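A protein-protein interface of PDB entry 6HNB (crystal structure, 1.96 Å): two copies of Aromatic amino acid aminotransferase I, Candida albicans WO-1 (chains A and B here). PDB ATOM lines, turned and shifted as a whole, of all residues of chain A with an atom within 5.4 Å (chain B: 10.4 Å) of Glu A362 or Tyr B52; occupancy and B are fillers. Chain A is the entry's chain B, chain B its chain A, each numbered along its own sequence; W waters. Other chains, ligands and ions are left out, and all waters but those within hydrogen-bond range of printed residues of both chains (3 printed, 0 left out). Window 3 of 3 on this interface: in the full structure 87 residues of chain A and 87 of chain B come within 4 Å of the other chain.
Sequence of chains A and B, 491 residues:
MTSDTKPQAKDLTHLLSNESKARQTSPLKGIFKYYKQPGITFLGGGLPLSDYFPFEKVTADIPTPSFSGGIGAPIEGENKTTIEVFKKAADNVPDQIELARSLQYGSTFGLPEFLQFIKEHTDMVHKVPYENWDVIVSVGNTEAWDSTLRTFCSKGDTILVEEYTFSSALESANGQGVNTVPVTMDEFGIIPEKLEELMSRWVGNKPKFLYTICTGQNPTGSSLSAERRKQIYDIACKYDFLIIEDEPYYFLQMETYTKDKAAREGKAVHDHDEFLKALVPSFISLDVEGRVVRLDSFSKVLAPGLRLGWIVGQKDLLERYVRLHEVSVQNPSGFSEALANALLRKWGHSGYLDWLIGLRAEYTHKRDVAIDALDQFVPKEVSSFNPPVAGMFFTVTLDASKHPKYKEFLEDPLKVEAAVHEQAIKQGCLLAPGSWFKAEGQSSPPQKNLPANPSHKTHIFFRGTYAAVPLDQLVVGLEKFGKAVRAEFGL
Hydrophobic or aromatic side chains of chain A within 4 Å of the printed part of chain B: Ile A71, Leu A302 and Trp A355. Of the 15 printed residues of chain B, 4 touch a printed residue of chain A. Among the printed residues, 9 pairs touch across the chains. Among the printed residues, no Asp or Glu carboxylate lies within 4 Å of a Lys or Arg side-chain nitrogen of the other chain.
Among the printed residues, merely in contact across the chains: Leu A302 with Pro B54 (3.2 Å), Trp A355 with Tyr B52 (3.3 Å), Leu A302 with Phe B53 (3.5 Å), Ile A71 with Tyr B52 (3.6 Å), Gly A72 with Tyr B52 (3.7 Å), Lys A366 with Leu B49 (3.9 Å) and Trp A355 with Pro B54 (3.9 Å).
Printed residues of chain B within 4 Å of Glu A362: Tyr B52. Of the printed residues of chain A, Tyr B52 touches Ile A71 (3.6 Å), Gly A72 (3.7 Å), Trp A355 (3.3 Å), Glu A362 (3.0 Å) and Lys A366 (2.9 Å). No residue of chain B comes within 4 Å of Gly A70. Ile A71 touches just one residue of chain B: Tyr B52. Of chain B, only Tyr B52 (3.7 Å) comes within 4 Å of Gly A72. No residue of chain B comes within 4 Å of Gly A358. Of the printed residues of chain B, Leu A302 touches Phe B53 and Pro B54. Of the printed residues of chain B, Lys A366 touches Leu B49 (3.9 Å) and Tyr B52 (2.9 Å). Ala B100 touches none of the printed residues of chain A. The nearest residue of chain B that does not touch Glu A362 is Leu B49 (6.7 Å). The nearest residue of chain A that does not touch Tyr B52 is Tyr A363 (4.4 Å). The nearest printed residue of chain B that does not touch Leu A302 is Tyr B52 (4.5 Å).
Water W1 lies within hydrogen-bond range of the backbone carbonyl oxygen of Ile A71 (2.7 Å) and the backbone carbonyl oxygen of Tyr B52 (3.2 Å). Water W3 bridges OH of Tyr A363 and N of Leu B49. Water W2 lies within hydrogen-bond range of the backbone carbonyl oxygen (O) of Asp B51 (3.1 Å) and the backbone carbonyl oxygen (O) of Gly A72 (3.4 Å).
The side-chain hydroxyl of Tyr B52 is in hydrogen-bond range of the side-chain amino group of Lys A366 (2.9 Å). OH of Tyr B52 lies within hydrogen-bond range of OE1 of Glu A362 (3.0 Å).
O of Phe B53 is in hydrogen-bond range of NZ of Lys B87 (2.7 Å).
No position is printed for both chains.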
ATOM      1  N   GLY A  70      33.514 -24.940 -17.039  1.00  0.00           N
ATOM      2  CA  GLY A  70      32.550 -24.228 -17.904  1.00  0.00           C
ATOM      3  C   GLY A  70      31.764 -23.196 -17.101  1.00  0.00           C
ATOM      4  O   GLY A  70      31.501 -23.444 -15.922  1.00  0.00           O
ATOM      5  N   ILE A  71      31.401 -22.069 -17.716  1.00  0.00           N
ATOM      6  CA  ILE A  71      30.743 -20.925 -17.008  1.00  0.00           C
ATOM      7  C   ILE A  71      29.372 -21.374 -16.472  1.00  0.00           C
ATOM      8  O   ILE A  71      28.875 -20.747 -15.520  1.00  0.00           O
ATOM      9  CB  ILE A  71      30.671 -19.673 -17.913  1.00  0.00           C
ATOM     10  CG1 ILE A  71      29.904 -19.950 -19.204  1.00  0.00           C
ATOM     11  CG2 ILE A  71      32.070 -19.132 -18.181  1.00  0.00           C
ATOM     12  CD1 ILE A  71      29.131 -18.752 -19.740  1.00  0.00           C
ATOM     13  N   GLY A  72      28.795 -22.440 -17.028  1.00  0.00           N
ATOM     14  CA  GLY A  72      27.513 -23.020 -16.575  1.00  0.00           C
ATOM     15  C   GLY A  72      27.668 -24.034 -15.439  1.00  0.00           C
ATOM     16  O   GLY A  72      26.656 -24.592 -15.038  1.00  0.00           O
ATOM     17  N   LEU A 302      26.382 -11.168 -17.951  1.00  0.00           N
ATOM     18  CA  LEU A 302      26.126 -11.598 -16.557  1.00  0.00           C
ATOM     19  C   LEU A 302      24.651 -11.965 -16.408  1.00  0.00           C
ATOM     20  O   LEU A 302      24.393 -13.168 -16.267  1.00  0.00           O
ATOM     21  CB  LEU A 302      26.550 -10.479 -15.607  1.00  0.00           C
ATOM     22  CG  LEU A 302      28.005 -10.025 -15.728  1.00  0.00           C
ATOM     23  CD1 LEU A 302      28.278  -8.956 -14.687  1.00  0.00           C
ATOM     24  CD2 LEU A 302      28.973 -11.191 -15.568  1.00  0.00           C
ATOM     25  N   TRP A 355      35.921 -15.205 -17.992  1.00  0.00           N
ATOM     26  CA  TRP A 355      34.452 -15.320 -18.125  1.00  0.00           C
ATOM     27  C   TRP A 355      34.063 -15.122 -19.593  1.00  0.00           C
ATOM     28  O   TRP A 355      33.352 -15.989 -20.140  1.00  0.00           O
ATOM     29  CB  TRP A 355      33.741 -14.328 -17.208  1.00  0.00           C
ATOM     30  CG  TRP A 355      32.251 -14.450 -17.328  1.00  0.00           C
ATOM     31  CD1 TRP A 355      31.431 -13.655 -18.067  1.00  0.00           C
ATOM     32  CD2 TRP A 355      31.415 -15.446 -16.723  1.00  0.00           C
ATOM     33  NE1 TRP A 355      30.137 -14.074 -17.936  1.00  0.00           N
ATOM     34  CE2 TRP A 355      30.088 -15.156 -17.106  1.00  0.00           C
ATOM     35  CE3 TRP A 355      31.640 -16.513 -15.842  1.00  0.00           C
ATOM     36  CZ2 TRP A 355      28.997 -15.932 -16.687  1.00  0.00           C
ATOM     37  CZ3 TRP A 355      30.568 -17.271 -15.426  1.00  0.00           C
ATOM     38  CH2 TRP A 355      29.260 -16.980 -15.834  1.00  0.00           C
ATOM     39  N   ILE A 357      35.864 -15.520 -22.220  1.00  0.00           N
ATOM     40  CA  ILE A 357      36.426 -16.652 -23.014  1.00  0.00           C
ATOM     41  C   ILE A 357      35.528 -17.886 -22.851  1.00  0.00           C
ATOM     42  O   ILE A 357      35.276 -18.568 -23.860  1.00  0.00           O
ATOM     43  CB  ILE A 357      37.914 -16.873 -22.648  1.00  0.00           C
ATOM     44  CG1 ILE A 357      38.762 -15.736 -23.217  1.00  0.00           C
ATOM     45  CG2 ILE A 357      38.423 -18.245 -23.096  1.00  0.00           C
ATOM     46  CD1 ILE A 357      40.081 -15.505 -22.502  1.00  0.00           C
ATOM     47  N   GLY A 358      35.013 -18.166 -21.657  1.00  0.00           N
ATOM     48  CA  GLY A 358      34.028 -19.248 -21.467  1.00  0.00           C
ATOM     49  C   GLY A 358      32.727 -18.981 -22.234  1.00  0.00           C
ATOM     50  O   GLY A 358      32.115 -19.934 -22.748  1.00  0.00           O
ATOM     51  N   LEU A 359      32.258 -17.735 -22.235  1.00  0.00           N
ATOM     52  CA  LEU A 359      31.046 -17.314 -22.962  1.00  0.00           C
ATOM     53  C   LEU A 359      31.257 -17.634 -24.442  1.00  0.00           C
ATOM     54  O   LEU A 359      30.359 -18.278 -25.054  1.00  0.00           O
ATOM     55  CB  LEU A 359      30.853 -15.819 -22.704  1.00  0.00           C
ATOM     56  CG  LEU A 359      29.459 -15.263 -22.951  1.00  0.00           C
ATOM     57  CD1 LEU A 359      28.417 -16.099 -22.233  1.00  0.00           C
ATOM     58  CD2 LEU A 359      29.396 -13.800 -22.492  1.00  0.00           C
ATOM     59  N   ARG A 360      32.420 -17.250 -24.974  1.00  0.00           N
ATOM     60  CA  ARG A 360      32.828 -17.481 -26.390  1.00  0.00           C
ATOM     61  C   ARG A 360      32.769 -18.985 -26.704  1.00  0.00           C
ATOM     62  O   ARG A 360      32.149 -19.332 -27.717  1.00  0.00           O
ATOM     63  CB  ARG A 360      34.197 -16.855 -26.659  1.00  0.00           C
ATOM     64  CG  ARG A 360      34.779 -17.153 -28.033  1.00  0.00           C
ATOM     65  CD  ARG A 360      36.194 -16.687 -28.199  1.00  0.00           C
ATOM     66  NE  ARG A 360      36.692 -16.787 -29.570  1.00  0.00           N
ATOM     67  CZ  ARG A 360      36.606 -15.829 -30.492  1.00  0.00           C
ATOM     68  NH1 ARG A 360      35.957 -14.699 -30.257  1.00  0.00           N
ATOM     69  NH2 ARG A 360      37.139 -16.025 -31.675  1.00  0.00           N
ATOM     70  N   ALA A 361      33.333 -19.844 -25.845  1.00  0.00           N
ATOM     71  CA  ALA A 361      33.351 -21.322 -26.013  1.00  0.00           C
ATOM     72  C   ALA A 361      31.922 -21.885 -25.999  1.00  0.00           C
ATOM     73  O   ALA A 361      31.626 -22.721 -26.891  1.00  0.00           O
ATOM     74  CB  ALA A 361      34.216 -21.977 -24.952  1.00  0.00           C
ATOM     75  N   GLU A 362      31.073 -21.458 -25.053  1.00  0.00           N
ATOM     76  CA  GLU A 362      29.682 -21.963 -24.915  1.00  0.00           C
ATOM     77  C   GLU A 362      28.876 -21.626 -26.181  1.00  0.00           C
ATOM     78  O   GLU A 362      28.137 -22.496 -26.656  1.00  0.00           O
ATOM     79  CB  GLU A 362      28.975 -21.367 -23.702  1.00  0.00           C
ATOM     80  CG  GLU A 362      29.550 -21.817 -22.383  1.00  0.00           C
ATOM     81  CD  GLU A 362      29.385 -23.303 -22.112  1.00  0.00           C
ATOM     82  OE1 GLU A 362      28.360 -23.871 -22.527  1.00  0.00           O
ATOM     83  OE2 GLU A 362      30.278 -23.879 -21.477  1.00  0.00           O
ATOM     84  N   TYR A 363      29.004 -20.415 -26.715  1.00  0.00           N
ATOM     85  CA  TYR A 363      28.181 -19.923 -27.843  1.00  0.00           C
ATOM     86  C   TYR A 363      28.720 -20.544 -29.130  1.00  0.00           C
ATOM     87  O   TYR A 363      27.916 -20.928 -29.984  1.00  0.00           O
ATOM     88  CB  TYR A 363      28.123 -18.387 -27.854  1.00  0.00           C
ATOM     89  CG  TYR A 363      26.979 -17.832 -27.049  1.00  0.00           C
ATOM     90  CD1 TYR A 363      27.052 -17.731 -25.680  1.00  0.00           C
ATOM     91  CD2 TYR A 363      25.807 -17.402 -27.669  1.00  0.00           C
ATOM     92  CE1 TYR A 363      25.999 -17.221 -24.945  1.00  0.00           C
ATOM     93  CE2 TYR A 363      24.760 -16.859 -26.953  1.00  0.00           C
ATOM     94  CZ  TYR A 363      24.854 -16.788 -25.581  1.00  0.00           C
ATOM     95  OH  TYR A 363      23.810 -16.329 -24.855  1.00  0.00           O
ATOM     96  N   THR A 364      30.034 -20.638 -29.285  1.00  0.00           N
ATOM     97  CA  THR A 364      30.640 -21.330 -30.447  1.00  0.00           C
ATOM     98  C   THR A 364      30.000 -22.721 -30.600  1.00  0.00           C
ATOM     99  O   THR A 364      29.551 -23.056 -31.703  1.00  0.00           O
ATOM    100  CB  THR A 364      32.156 -21.426 -30.318  1.00  0.00           C
ATOM    101  OG1 THR A 364      32.662 -20.094 -30.404  1.00  0.00           O
ATOM    102  CG2 THR A 364      32.752 -22.288 -31.405  1.00  0.00           C
ATOM    103  N   HIS A 365      29.875 -23.479 -29.516  1.00  0.00           N
ATOM    104  CA  HIS A 365      29.329 -24.855 -29.586  1.00  0.00           C
ATOM    105  C   HIS A 365      27.847 -24.813 -30.008  1.00  0.00           C
ATOM    106  O   HIS A 365      27.489 -25.585 -30.916  1.00  0.00           O
ATOM    107  CB  HIS A 365      29.540 -25.618 -28.282  1.00  0.00           C
ATOM    108  CG  HIS A 365      29.035 -27.019 -28.403  1.00  0.00           C
ATOM    109  ND1 HIS A 365      29.482 -27.876 -29.396  1.00  0.00           N
ATOM    110  CD2 HIS A 365      28.099 -27.690 -27.703  1.00  0.00           C
ATOM    111  CE1 HIS A 365      28.839 -29.019 -29.283  1.00  0.00           C
ATOM    112  NE2 HIS A 365      27.982 -28.926 -28.260  1.00  0.00           N
ATOM    113  N   LYS A 366      27.038 -23.925 -29.415  1.00  0.00           N
ATOM    114  CA  LYS A 366      25.576 -23.817 -29.725  1.00  0.00           C
ATOM    115  C   LYS A 366      25.362 -23.527 -31.212  1.00  0.00           C
ATOM    116  O   LYS A 366      24.471 -24.147 -31.804  1.00  0.00           O
ATOM    117  CB  LYS A 366      24.916 -22.721 -28.891  1.00  0.00           C
ATOM    118  CG  LYS A 366      24.855 -22.961 -27.390  1.00  0.00           C
ATOM    119  CD  LYS A 366      24.274 -21.768 -26.679  1.00  0.00           C
ATOM    120  CE  LYS A 366      24.558 -21.761 -25.199  1.00  0.00           C
ATOM    121  NZ  LYS A 366      23.980 -22.959 -24.556  1.00  0.00           N
ATOM    122  N   LEU B  47      15.929 -14.587 -25.189  1.00  0.00           N
ATOM    123  CA  LEU B  47      16.315 -14.741 -23.761  1.00  0.00           C
ATOM    124  C   LEU B  47      17.652 -15.476 -23.663  1.00  0.00           C
ATOM    125  O   LEU B  47      17.770 -16.597 -24.143  1.00  0.00           O
ATOM    126  CB  LEU B  47      15.230 -15.530 -23.023  1.00  0.00           C
ATOM    127  CG  LEU B  47      13.862 -14.857 -22.881  1.00  0.00           C
ATOM    128  CD1 LEU B  47      12.941 -15.720 -22.020  1.00  0.00           C
ATOM    129  CD2 LEU B  47      13.967 -13.440 -22.305  1.00  0.00           C
ATOM    130  N   PRO B  48      18.696 -14.895 -23.034  1.00  0.00           N
ATOM    131  CA  PRO B  48      19.894 -15.665 -22.708  1.00  0.00           C
ATOM    132  C   PRO B  48      19.577 -16.708 -21.616  1.00  0.00           C
ATOM    133  O   PRO B  48      18.495 -16.682 -21.013  1.00  0.00           O
ATOM    134  CB  PRO B  48      20.926 -14.607 -22.278  1.00  0.00           C
ATOM    135  CG  PRO B  48      20.091 -13.439 -21.785  1.00  0.00           C
ATOM    136  CD  PRO B  48      18.799 -13.491 -22.592  1.00  0.00           C
ATOM    137  N   LEU B  49      20.517 -17.633 -21.406  1.00  0.00           N
ATOM    138  CA  LEU B  49      20.288 -18.880 -20.629  1.00  0.00           C
ATOM    139  C   LEU B  49      20.563 -18.573 -19.159  1.00  0.00           C
ATOM    140  O   LEU B  49      21.689 -18.079 -18.853  1.00  0.00           O
ATOM    141  CB  LEU B  49      21.211 -19.977 -21.182  1.00  0.00           C
ATOM    142  CG  LEU B  49      20.938 -21.396 -20.694  1.00  0.00           C
ATOM    143  CD1 LEU B  49      19.530 -21.860 -21.076  1.00  0.00           C
ATOM    144  CD2 LEU B  49      22.003 -22.341 -21.251  1.00  0.00           C
ATOM    145  N   SER B  50      19.576 -18.821 -18.295  1.00  0.00           N
ATOM    146  CA  SER B  50      19.669 -18.530 -16.842  1.00  0.00           C
ATOM    147  C   SER B  50      20.750 -19.419 -16.212  1.00  0.00           C
ATOM    148  O   SER B  50      21.236 -19.067 -15.117  1.00  0.00           O
ATOM    149  CB  SER B  50      18.318 -18.666 -16.165  1.00  0.00           C
ATOM    150  OG  SER B  50      17.970 -20.026 -15.942  1.00  0.00           O
ATOM    151  N   ASP B  51      21.137 -20.511 -16.896  1.00  0.00           N
ATOM    152  CA  ASP B  51      22.181 -21.472 -16.439  1.00  0.00           C
ATOM    153  C   ASP B  51      23.488 -20.716 -16.193  1.00  0.00           C
ATOM    154  O   ASP B  51      24.186 -21.085 -15.242  1.00  0.00           O
ATOM    155  CB  ASP B  51      22.449 -22.611 -17.428  1.00  0.00           C
ATOM    156  CG  ASP B  51      21.250 -23.477 -17.785  1.00  0.00           C
ATOM    157  OD1 ASP B  51      20.254 -23.452 -17.051  1.00  0.00           O
ATOM    158  OD2 ASP B  51      21.319 -24.157 -18.822  1.00  0.00           O
ATOM    159  N   TYR B  52      23.796 -19.681 -16.991  1.00  0.00           N
ATOM    160  CA  TYR B  52      25.074 -18.936 -16.887  1.00  0.00           C
ATOM    161  C   TYR B  52      24.981 -17.783 -15.877  1.00  0.00           C
ATOM    162  O   TYR B  52      26.026 -17.321 -15.490  1.00  0.00           O
ATOM    163  CB  TYR B  52      25.534 -18.430 -18.254  1.00  0.00           C
ATOM    164  CG  TYR B  52      25.614 -19.481 -19.335  1.00  0.00           C
ATOM    165  CD1 TYR B  52      25.994 -20.791 -19.061  1.00  0.00           C
ATOM    166  CD2 TYR B  52      25.336 -19.150 -20.650  1.00  0.00           C
ATOM    167  CE1 TYR B  52      26.035 -21.749 -20.058  1.00  0.00           C
ATOM    168  CE2 TYR B  52      25.406 -20.093 -21.666  1.00  0.00           C
ATOM    169  CZ  TYR B  52      25.756 -21.396 -21.367  1.00  0.00           C
ATOM    170  OH  TYR B  52      25.833 -22.307 -22.378  1.00  0.00           O
ATOM    171  N   PHE B  53      23.810 -17.324 -15.436  1.00  0.00           N
ATOM    172  CA  PHE B  53      23.761 -16.158 -14.510  1.00  0.00           C
ATOM    173  C   PHE B  53      24.728 -16.448 -13.357  1.00  0.00           C
ATOM    174  O   PHE B  53      24.558 -17.459 -12.666  1.00  0.00           O
ATOM    175  CB  PHE B  53      22.341 -15.860 -14.009  1.00  0.00           C
ATOM    176  CG  PHE B  53      21.302 -15.511 -15.049  1.00  0.00           C
ATOM    177  CD1 PHE B  53      21.629 -15.305 -16.384  1.00  0.00           C
ATOM    178  CD2 PHE B  53      19.963 -15.414 -14.684  1.00  0.00           C
ATOM    179  CE1 PHE B  53      20.645 -14.990 -17.321  1.00  0.00           C
ATOM    180  CE2 PHE B  53      18.978 -15.113 -15.625  1.00  0.00           C
ATOM    181  CZ  PHE B  53      19.324 -14.876 -16.939  1.00  0.00           C
ATOM    182  N   PRO B  54      25.804 -15.645 -13.149  1.00  0.00           N
ATOM    183  CA  PRO B  54      26.817 -15.944 -12.123  1.00  0.00           C
ATOM    184  C   PRO B  54      26.444 -15.524 -10.686  1.00  0.00           C
ATOM    185  O   PRO B  54      27.290 -15.084  -9.961  1.00  0.00           O
ATOM    186  CB  PRO B  54      28.020 -15.124 -12.608  1.00  0.00           C
ATOM    187  CG  PRO B  54      27.385 -13.897 -13.218  1.00  0.00           C
ATOM    188  CD  PRO B  54      26.171 -14.452 -13.927  1.00  0.00           C
ATOM    189  N   PHE B  55      25.183 -15.704 -10.295  1.00  0.00           N
ATOM    190  CA  PHE B  55      24.686 -15.426  -8.927  1.00  0.00           C
ATOM    191  C   PHE B  55      23.918 -16.650  -8.435  1.00  0.00           C
ATOM    192  O   PHE B  55      22.811 -16.888  -8.921  1.00  0.00           O
ATOM    193  CB  PHE B  55      23.845 -14.143  -8.919  1.00  0.00           C
ATOM    194  CG  PHE B  55      24.572 -12.944  -9.465  1.00  0.00           C
ATOM    195  CD1 PHE B  55      25.386 -12.173  -8.646  1.00  0.00           C
ATOM    196  CD2 PHE B  55      24.471 -12.613 -10.811  1.00  0.00           C
ATOM    197  CE1 PHE B  55      26.046 -11.061  -9.150  1.00  0.00           C
ATOM    198  CE2 PHE B  55      25.159 -11.521 -11.318  1.00  0.00           C
ATOM    199  CZ  PHE B  55      25.935 -10.747 -10.488  1.00  0.00           C
ATOM    200  N   GLU B  56      24.521 -17.439  -7.540  1.00  0.00           N
ATOM    201  CA  GLU B  56      23.851 -18.640  -6.958  1.00  0.00           C
ATOM    202  C   GLU B  56      22.856 -18.186  -5.875  1.00  0.00           C
ATOM    203  O   GLU B  56      21.842 -18.874  -5.630  1.00  0.00           O
ATOM    204  CB  GLU B  56      24.906 -19.617  -6.430  1.00  0.00           C
ATOM    205  CG  GLU B  56      24.339 -20.826  -5.705  1.00  0.00           C
ATOM    206  CD  GLU B  56      23.309 -21.643  -6.459  1.00  0.00           C
ATOM    207  OE1 GLU B  56      23.287 -21.562  -7.692  1.00  0.00           O
ATOM    208  OE2 GLU B  56      22.511 -22.355  -5.804  1.00  0.00           O
ATOM    209  N   LYS B  87      19.029 -18.780  -6.525  1.00  0.00           N
ATOM    210  CA  LYS B  87      18.795 -18.818  -7.991  1.00  0.00           C
ATOM    211  C   LYS B  87      17.580 -19.695  -8.320  1.00  0.00           C
ATOM    212  O   LYS B  87      16.808 -19.304  -9.213  1.00  0.00           O
ATOM    213  CB  LYS B  87      20.070 -19.320  -8.680  1.00  0.00           C
ATOM    214  CG  LYS B  87      20.039 -19.329 -10.199  1.00  0.00           C
ATOM    215  CD  LYS B  87      21.406 -19.642 -10.780  1.00  0.00           C
ATOM    216  CE  LYS B  87      21.446 -19.606 -12.285  1.00  0.00           C
ATOM    217  NZ  LYS B  87      22.851 -19.530 -12.772  1.00  0.00           N
ATOM    218  N   LEU B  99      16.454 -16.009  -8.362  1.00  0.00           N
ATOM    219  CA  LEU B  99      17.323 -15.210  -9.269  1.00  0.00           C
ATOM    220  C   LEU B  99      17.242 -15.733 -10.715  1.00  0.00           C
ATOM    221  O   LEU B  99      17.474 -14.909 -11.635  1.00  0.00           O
ATOM    222  CB  LEU B  99      18.766 -15.210  -8.741  1.00  0.00           C
ATOM    223  CG  LEU B  99      18.958 -14.677  -7.312  1.00  0.00           C
ATOM    224  CD1 LEU B  99      20.429 -14.665  -6.932  1.00  0.00           C
ATOM    225  CD2 LEU B  99      18.366 -13.276  -7.160  1.00  0.00           C
ATOM    226  N   ALA B 100      16.906 -17.012 -10.949  1.00  0.00           N
ATOM    227  CA  ALA B 100      16.704 -17.536 -12.328  1.00  0.00           C
ATOM    228  C   ALA B 100      15.611 -16.707 -13.034  1.00  0.00           C
ATOM    229  O   ALA B 100      15.726 -16.476 -14.251  1.00  0.00           O
ATOM    230  CB  ALA B 100      16.375 -19.025 -12.335  1.00  0.00           C
ATOM    231  N   LEU B 103      16.409 -12.308 -12.283  1.00  0.00           N
ATOM    232  CA  LEU B 103      17.509 -11.727 -13.118  1.00  0.00           C
ATOM    233  C   LEU B 103      17.302 -12.016 -14.607  1.00  0.00           C
ATOM    234  O   LEU B 103      18.221 -11.687 -15.370  1.00  0.00           O
ATOM    235  CB  LEU B 103      18.888 -12.230 -12.659  1.00  0.00           C
ATOM    236  CG  LEU B 103      19.266 -11.933 -11.209  1.00  0.00           C
ATOM    237  CD1 LEU B 103      20.633 -12.523 -10.899  1.00  0.00           C
ATOM    238  CD2 LEU B 103      19.227 -10.436 -10.894  1.00  0.00           C
ATOM    239  N   GLN B 104      16.144 -12.556 -15.021  1.00  0.00           N
ATOM    240  CA  GLN B 104      15.778 -12.790 -16.446  1.00  0.00           C
ATOM    241  C   GLN B 104      14.887 -11.622 -16.893  1.00  0.00           C
ATOM    242  O   GLN B 104      14.248 -10.993 -15.986  1.00  0.00           O
ATOM    243  CB  GLN B 104      15.041 -14.135 -16.612  1.00  0.00           C
ATOM    244  CG  GLN B 104      14.730 -14.552 -18.056  1.00  0.00           C
ATOM    245  CD  GLN B 104      15.934 -14.581 -18.972  1.00  0.00           C
ATOM    246  OE1 GLN B 104      16.344 -13.545 -19.518  1.00  0.00           O
ATOM    247  NE2 GLN B 104      16.491 -15.774 -19.179  1.00  0.00           N
HETATM  248  O   HOH W   1      27.426 -19.501 -13.627  1.00  0.00           O
HETATM  249  O   HOH W   2      26.329 -21.773 -13.180  1.00  0.00           O
HETATM  250  O   HOH W   3      22.436 -18.097 -23.303  1.00  0.00           O
